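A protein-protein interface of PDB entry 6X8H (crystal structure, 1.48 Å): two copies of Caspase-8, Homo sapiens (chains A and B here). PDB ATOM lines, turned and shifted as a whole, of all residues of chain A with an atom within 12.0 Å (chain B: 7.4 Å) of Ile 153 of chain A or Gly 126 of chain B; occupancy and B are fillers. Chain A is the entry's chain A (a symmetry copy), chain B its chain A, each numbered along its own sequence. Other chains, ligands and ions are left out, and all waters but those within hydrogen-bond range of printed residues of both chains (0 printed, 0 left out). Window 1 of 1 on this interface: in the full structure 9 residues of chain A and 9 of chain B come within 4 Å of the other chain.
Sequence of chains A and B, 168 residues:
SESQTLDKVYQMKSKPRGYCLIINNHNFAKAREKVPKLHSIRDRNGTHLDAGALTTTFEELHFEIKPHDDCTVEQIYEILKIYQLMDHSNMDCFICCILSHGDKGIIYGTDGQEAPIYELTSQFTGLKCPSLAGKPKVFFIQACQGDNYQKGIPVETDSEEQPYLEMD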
ATOM      1  N   TYR A 149      13.148  19.005 -15.707  1.00  0.00           N
ATOM      2  CA  TYR A 149      13.554  17.716 -16.232  1.00  0.00           C
ATOM      3  C   TYR A 149      13.159  17.628 -17.705  1.00  0.00           C
ATOM      4  O   TYR A 149      12.062  18.026 -18.103  1.00  0.00           O
ATOM      5  CB  TYR A 149      12.892  16.561 -15.463  1.00  0.00           C
ATOM      6  CG  TYR A 149      13.091  16.636 -13.974  1.00  0.00           C
ATOM      7  CD1 TYR A 149      14.324  16.961 -13.425  1.00  0.00           C
ATOM      8  CD2 TYR A 149      12.027  16.446 -13.107  1.00  0.00           C
ATOM      9  CE1 TYR A 149      14.491  17.042 -12.035  1.00  0.00           C
ATOM     10  CE2 TYR A 149      12.193  16.530 -11.736  1.00  0.00           C
ATOM     11  CZ  TYR A 149      13.407  16.844 -11.212  1.00  0.00           C
ATOM     12  OH  TYR A 149      13.560  16.942  -9.846  1.00  0.00           O
ATOM     13  N   GLN A 150      14.066  17.123 -18.519  1.00  0.00           N
ATOM     14  CA  GLN A 150      13.770  16.890 -19.928  1.00  0.00           C
ATOM     15  C   GLN A 150      12.949  15.602 -20.020  1.00  0.00           C
ATOM     16  O   GLN A 150      13.378  14.548 -19.536  1.00  0.00           O
ATOM     17  CB  GLN A 150      15.098  16.777 -20.668  1.00  0.00           C
ATOM     18  CG  GLN A 150      14.972  16.448 -22.112  1.00  0.00           C
ATOM     19  CD  GLN A 150      14.496  17.596 -23.018  1.00  0.00           C
ATOM     20  OE1 GLN A 150      14.424  18.796 -22.663  1.00  0.00           O
ATOM     21  NE2 GLN A 150      14.148  17.221 -24.197  1.00  0.00           N
ATOM     22  N   LYS A 151      11.772  15.670 -20.636  1.00  0.00           N
ATOM     23  CA  LYS A 151      10.931  14.485 -20.771  1.00  0.00           C
ATOM     24  C   LYS A 151      11.426  13.530 -21.872  1.00  0.00           C
ATOM     25  O   LYS A 151      12.162  13.901 -22.792  1.00  0.00           O
ATOM     26  CB  LYS A 151       9.476  14.899 -21.038  1.00  0.00           C
ATOM     27  CG  LYS A 151       8.812  15.671 -19.917  1.00  0.00           C
ATOM     28  CD  LYS A 151       7.368  15.977 -20.276  1.00  0.00           C
ATOM     29  CE  LYS A 151       6.705  16.951 -19.307  1.00  0.00           C
ATOM     30  NZ  LYS A 151       7.307  18.318 -19.343  1.00  0.00           N
ATOM     31  N   GLY A 152      11.044  12.262 -21.741  1.00  0.00           N
ATOM     32  CA  GLY A 152      11.338  11.266 -22.747  1.00  0.00           C
ATOM     33  C   GLY A 152      10.186  11.050 -23.719  1.00  0.00           C
ATOM     34  O   GLY A 152       9.031  11.328 -23.408  1.00  0.00           O
ATOM     35  N   ILE A 153      10.527  10.562 -24.914  1.00  0.00           N
ATOM     36  CA  ILE A 153       9.548  10.212 -25.951  1.00  0.00           C
ATOM     37  C   ILE A 153       9.838   8.802 -26.447  1.00  0.00           C
ATOM     38  O   ILE A 153      11.010   8.412 -26.582  1.00  0.00           O
ATOM     39  CB  ILE A 153       9.557  11.221 -27.123  1.00  0.00           C
ATOM     40  CG1 ILE A 153      10.963  11.331 -27.750  1.00  0.00           C
ATOM     41  CG2 ILE A 153       9.074  12.546 -26.613  1.00  0.00           C
ATOM     42  CD1 ILE A 153      11.078  12.252 -28.975  1.00  0.00           C
ATOM     43  N   PRO A 154       8.811   8.002 -26.742  1.00  0.00           N
ATOM     44  CA  PRO A 154       9.050   6.630 -27.189  1.00  0.00           C
ATOM     45  C   PRO A 154       9.359   6.580 -28.683  1.00  0.00           C
ATOM     46  O   PRO A 154       8.725   7.254 -29.494  1.00  0.00           O
ATOM     47  CB  PRO A 154       7.717   5.941 -26.870  1.00  0.00           C
ATOM     48  CG  PRO A 154       6.716   7.042 -27.016  1.00  0.00           C
ATOM     49  CD  PRO A 154       7.385   8.278 -26.480  1.00  0.00           C
ATOM     50  N   VAL A 155      10.376   5.790 -29.037  1.00  0.00           N
ATOM     51  CA  VAL A 155      10.758   5.592 -30.437  1.00  0.00           C
ATOM     52  C   VAL A 155      11.108   4.126 -30.681  1.00  0.00           C
ATOM     53  O   VAL A 155      11.421   3.375 -29.756  1.00  0.00           O
ATOM     54  CB  VAL A 155      11.948   6.503 -30.841  1.00  0.00           C
ATOM     55  CG1 VAL A 155      11.558   8.015 -30.836  1.00  0.00           C
ATOM     56  CG2 VAL A 155      13.152   6.252 -29.930  1.00  0.00           C
ATOM     57  N   GLU A 156      11.104   3.728 -31.950  1.00  0.00           N
ATOM     58  CA  GLU A 156      11.544   2.370 -32.276  1.00  0.00           C
ATOM     59  C   GLU A 156      13.060   2.224 -32.126  1.00  0.00           C
ATOM     60  O   GLU A 156      13.835   3.159 -32.369  1.00  0.00           O
ATOM     61  CB  GLU A 156      11.066   1.932 -33.673  1.00  0.00           C
ATOM     62  N   THR A 157      13.481   1.038 -31.678  1.00  0.00           N
ATOM     63  CA  THR A 157      14.901   0.771 -31.457  1.00  0.00           C
ATOM     64  C   THR A 157      15.647   0.703 -32.789  1.00  0.00           C
ATOM     65  O   THR A 157      15.101   0.277 -33.813  1.00  0.00           O
ATOM     66  CB  THR A 157      15.083  -0.541 -30.682  1.00  0.00           C
ATOM     67  OG1 THR A 157      16.448  -0.672 -30.258  1.00  0.00           O
ATOM     68  CG2 THR A 157      14.738  -1.734 -31.551  1.00  0.00           C
ATOM     69  N   ASP A 158      16.905   1.154 -32.773  1.00  0.00           N
ATOM     70  CA  ASP A 158      17.813   1.047 -33.930  1.00  0.00           C
ATOM     71  C   ASP A 158      18.276  -0.398 -34.098  1.00  0.00           C
ATOM     72  O   ASP A 158      18.280  -1.146 -33.116  1.00  0.00           O
ATOM     73  CB  ASP A 158      19.045   1.923 -33.715  1.00  0.00           C
ATOM     74  CG  ASP A 158      18.780   3.383 -34.010  1.00  0.00           C
ATOM     75  OD1 ASP A 158      17.874   3.677 -34.804  1.00  0.00           O
ATOM     76  OD2 ASP A 158      19.473   4.222 -33.415  1.00  0.00           O
ATOM     77  N   SER B 122       9.913  24.597 -30.674  1.00  0.00           N
ATOM     78  CA  SER B 122       9.302  23.691 -29.711  1.00  0.00           C
ATOM     79  C   SER B 122       7.894  23.252 -30.104  1.00  0.00           C
ATOM     80  O   SER B 122       7.331  22.388 -29.432  1.00  0.00           O
ATOM     81  CB  SER B 122       9.362  24.247 -28.290  1.00  0.00           C
ATOM     82  OG  SER B 122       8.572  25.405 -28.166  1.00  0.00           O
ATOM     83  N   GLN B 123       7.314  23.791 -31.177  1.00  0.00           N
ATOM     84  CA  GLN B 123       6.071  23.191 -31.644  1.00  0.00           C
ATOM     85  C   GLN B 123       6.280  21.801 -32.228  1.00  0.00           C
ATOM     86  O   GLN B 123       5.296  21.096 -32.456  1.00  0.00           O
ATOM     87  CB  GLN B 123       5.372  24.080 -32.690  1.00  0.00           C
ATOM     88  CG  GLN B 123       5.058  25.500 -32.177  1.00  0.00           C
ATOM     89  CD  GLN B 123       4.379  25.489 -30.823  1.00  0.00           C
ATOM     90  OE1 GLN B 123       3.422  24.748 -30.597  1.00  0.00           O
ATOM     91  NE2 GLN B 123       4.891  26.296 -29.894  1.00  0.00           N
ATOM     92  N   PHE B 124       7.521  21.371 -32.458  1.00  0.00           N
ATOM     93  CA  PHE B 124       7.777  20.119 -33.154  1.00  0.00           C
ATOM     94  C   PHE B 124       8.564  19.143 -32.305  1.00  0.00           C
ATOM     95  O   PHE B 124       9.186  18.223 -32.842  1.00  0.00           O
ATOM     96  CB  PHE B 124       8.434  20.343 -34.515  1.00  0.00           C
ATOM     97  CG  PHE B 124       7.574  21.126 -35.433  1.00  0.00           C
ATOM     98  CD1 PHE B 124       7.572  22.517 -35.362  1.00  0.00           C
ATOM     99  CD2 PHE B 124       6.683  20.480 -36.270  1.00  0.00           C
ATOM    100  CE1 PHE B 124       6.720  23.249 -36.167  1.00  0.00           C
ATOM    101  CE2 PHE B 124       5.838  21.209 -37.096  1.00  0.00           C
ATOM    102  CZ  PHE B 124       5.854  22.592 -37.019  1.00  0.00           C
ATOM    103  N   THR B 125       8.510  19.314 -30.988  1.00  0.00           N
ATOM    104  CA  THR B 125       9.127  18.320 -30.114  1.00  0.00           C
ATOM    105  C   THR B 125       8.445  16.977 -30.292  1.00  0.00           C
ATOM    106  O   THR B 125       7.347  16.862 -30.866  1.00  0.00           O
ATOM    107  CB  THR B 125       9.059  18.714 -28.648  1.00  0.00           C
ATOM    108  OG1 THR B 125       7.697  18.808 -28.240  1.00  0.00           O
ATOM    109  CG2 THR B 125       9.815  20.053 -28.359  1.00  0.00           C
ATOM    110  N   GLY B 126       9.107  15.943 -29.773  1.00  0.00           N
ATOM    111  CA  GLY B 126       8.545  14.611 -29.909  1.00  0.00           C
ATOM    112  C   GLY B 126       7.165  14.472 -29.285  1.00  0.00           C
ATOM    113  O   GLY B 126       6.339  13.696 -29.773  1.00  0.00           O
ATOM    114  N   LEU B 127       6.904  15.173 -28.178  1.00  0.00           N
ATOM    115  CA  LEU B 127       5.602  15.081 -27.526  1.00  0.00           C
ATOM    116  C   LEU B 127       4.547  15.827 -28.305  1.00  0.00           C
ATOM    117  O   LEU B 127       3.411  15.363 -28.390  1.00  0.00           O
ATOM    118  CB  LEU B 127       5.681  15.652 -26.109  1.00  0.00           C
ATOM    119  CG  LEU B 127       6.509  14.798 -25.125  1.00  0.00           C
ATOM    120  CD1 LEU B 127       6.827  15.557 -23.805  1.00  0.00           C
ATOM    121  CD2 LEU B 127       5.805  13.452 -24.823  1.00  0.00           C
ATOM    122  N   LYS B 128       4.886  17.004 -28.850  1.00  0.00           N
ATOM    123  CA  LYS B 128       3.898  17.762 -29.630  1.00  0.00           C
ATOM    124  C   LYS B 128       3.638  17.170 -31.012  1.00  0.00           C
ATOM    125  O   LYS B 128       2.516  17.298 -31.529  1.00  0.00           O
ATOM    126  CB  LYS B 128       4.309  19.232 -29.730  1.00  0.00           C
ATOM    127  CG  LYS B 128       4.405  19.856 -28.340  1.00  0.00           C
ATOM    128  CD  LYS B 128       4.187  21.363 -28.280  1.00  0.00           C
ATOM    129  CE  LYS B 128       5.044  22.131 -27.177  1.00  0.00           C
ATOM    130  NZ  LYS B 128       6.548  21.782 -26.948  1.00  0.00           N
ATOM    131  N   CYS B 129       4.637  16.519 -31.609  1.00  0.00           N
ATOM    132  CA  CYS B 129       4.521  15.945 -32.952  1.00  0.00           C
ATOM    133  C   CYS B 129       5.123  14.548 -32.929  1.00  0.00           C
ATOM    134  O   CYS B 129       6.249  14.335 -33.418  1.00  0.00           O
ATOM    135  CB  CYS B 129       5.243  16.831 -33.969  1.00  0.00           C
ATOM    136  SG  CYS B 129       4.774  16.329 -35.675  1.00  0.00           S
ATOM    137  N   PRO B 130       4.403  13.554 -32.396  1.00  0.00           N
ATOM    138  CA  PRO B 130       4.984  12.194 -32.318  1.00  0.00           C
ATOM    139  C   PRO B 130       5.270  11.565 -33.649  1.00  0.00           C
ATOM    140  O   PRO B 130       6.148  10.693 -33.739  1.00  0.00           O
ATOM    141  CB  PRO B 130       3.923  11.386 -31.544  1.00  0.00           C
ATOM    142  CG  PRO B 130       3.250  12.436 -30.680  1.00  0.00           C
ATOM    143  CD  PRO B 130       3.178  13.671 -31.579  1.00  0.00           C
ATOM    144  N   SER B 131       4.562  11.963 -34.710  1.00  0.00           N
ATOM    145  CA  SER B 131       4.864  11.362 -35.997  1.00  0.00           C
ATOM    146  C   SER B 131       6.196  11.831 -36.560  1.00  0.00           C
ATOM    147  O   SER B 131       6.608  11.299 -37.594  1.00  0.00           O
ATOM    148  CB  SER B 131       3.721  11.576 -36.986  1.00  0.00           C
ATOM    149  OG  SER B 131       3.469  12.946 -37.236  1.00  0.00           O
ATOM    150  N   LEU B 132       6.873  12.794 -35.916  1.00  0.00           N
ATOM    151  CA  LEU B 132       8.249  13.153 -36.266  1.00  0.00           C
ATOM    152  C   LEU B 132       9.252  12.695 -35.201  1.00  0.00           C
ATOM    153  O   LEU B 132      10.439  13.008 -35.294  1.00  0.00           O
ATOM    154  CB  LEU B 132       8.369  14.667 -36.496  1.00  0.00           C
ATOM    155  CG  LEU B 132       7.807  15.243 -37.784  1.00  0.00           C
ATOM    156  CD1 LEU B 132       7.802  16.819 -37.788  1.00  0.00           C
ATOM    157  CD2 LEU B 132       8.572  14.718 -38.979  1.00  0.00           C
ATOM    158  N   ALA B 133       8.802  11.947 -34.202  1.00  0.00           N
ATOM    159  CA  ALA B 133       9.705  11.472 -33.160  1.00  0.00           C
ATOM    160  C   ALA B 133      10.809  10.578 -33.737  1.00  0.00           C
ATOM    161  O   ALA B 133      10.564   9.650 -34.527  1.00  0.00           O
ATOM    162  CB  ALA B 133       8.917  10.729 -32.059  1.00  0.00           C
ATOM    163  N   GLY B 134      12.052  10.856 -33.337  1.00  0.00           N
ATOM    164  CA  GLY B 134      13.172  10.125 -33.888  1.00  0.00           C
ATOM    165  C   GLY B 134      13.626  10.610 -35.230  1.00  0.00           C
ATOM    166  O   GLY B 134      14.604  10.065 -35.758  1.00  0.00           O
ATOM    167  N   LYS B 135      12.936  11.635 -35.811  1.00  0.00           N
ATOM    168  CA  LYS B 135      13.231  12.080 -37.155  1.00  0.00           C
ATOM    169  C   LYS B 135      13.800  13.496 -37.125  1.00  0.00           C
ATOM    170  O   LYS B 135      13.436  14.312 -36.258  1.00  0.00           O
ATOM    171  CB  LYS B 135      11.992  12.037 -38.054  1.00  0.00           C
ATOM    172  CG  LYS B 135      11.346  10.643 -38.153  1.00  0.00           C
ATOM    173  CD  LYS B 135      10.045  10.753 -38.924  1.00  0.00           C
ATOM    174  CE  LYS B 135       9.288   9.444 -38.901  1.00  0.00           C
ATOM    175  NZ  LYS B 135       7.973   9.609 -39.571  1.00  0.00           N
ATOM    176  N   LYS B 137      14.433  17.301 -37.523  1.00  0.00           N
ATOM    177  CA  LYS B 137      13.628  18.513 -37.680  1.00  0.00           C
ATOM    178  C   LYS B 137      14.620  19.650 -37.858  1.00  0.00           C
ATOM    179  O   LYS B 137      15.438  19.907 -36.953  1.00  0.00           O
ATOM    180  CB  LYS B 137      12.809  18.754 -36.426  1.00  0.00           C
ATOM    181  CG  LYS B 137      11.656  17.698 -36.330  1.00  0.00           C
ATOM    182  CD  LYS B 137      11.171  17.517 -34.939  1.00  0.00           C
ATOM    183  CE  LYS B 137      12.084  16.666 -34.094  1.00  0.00           C
ATOM    184  NZ  LYS B 137      11.716  15.207 -34.201  1.00  0.00           N
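Lys 151 of chain A touches Leu 127 of chain B. Gly 126 of chain B touches Ile 153 of chain A (CA to CD1, 3.6 Å). CG2 of Ile 153 of chain A touches CG of Leu 127 of chain B, at 3.7 Å. C of Ala 133 of chain B touches CG1 of Val 155 of chain A (3.9 Å). CG1 of Val 155 of chain A touches N of Gly 134 of chain B (3.8 Å).
Of the printed residues of chain B, Val 155 of chain A touches Ala 133 (3.9 Å) and Gly 134 (3.8 Å). Gly 126 of chain B touches just one residue of chain A: Ile 153 (3.6 Å). No residue of chain A comes within 4 Å of Lys 128 of chain B. No residue of chain A comes within 4 Å of Cys 129 of chain B. No residue of chain A comes within 4 Å of Pro 130 of chain B. Leu 132 of chain B touches none of the printed residues of chain A. Of the printed residues of chain A, Gly 134 of chain B touches Val 155. The nearest residue of chain B that does not touch Ile 153 of chain A is Ala 133 of chain B (4.1 Å). The nearest residue of chain A that does not touch Gly 126 of chain B is Pro 154 of chain A (6.4 Å).
Hydrophobic or aromatic side chains of chain A that line the printed part of chain B: Ile 153 and Val 155. Among the printed residues, 5 pairs touch across the chains. Among the printed residues, no Asp or Glu carboxylate lies within 4 Å of a Lys or Arg side-chain nitrogen of the other chain.
No position is printed for both chains. Of the 5 pairs that touch across the chains among the printed residues, none has its exchanged pair printed and touching as well.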
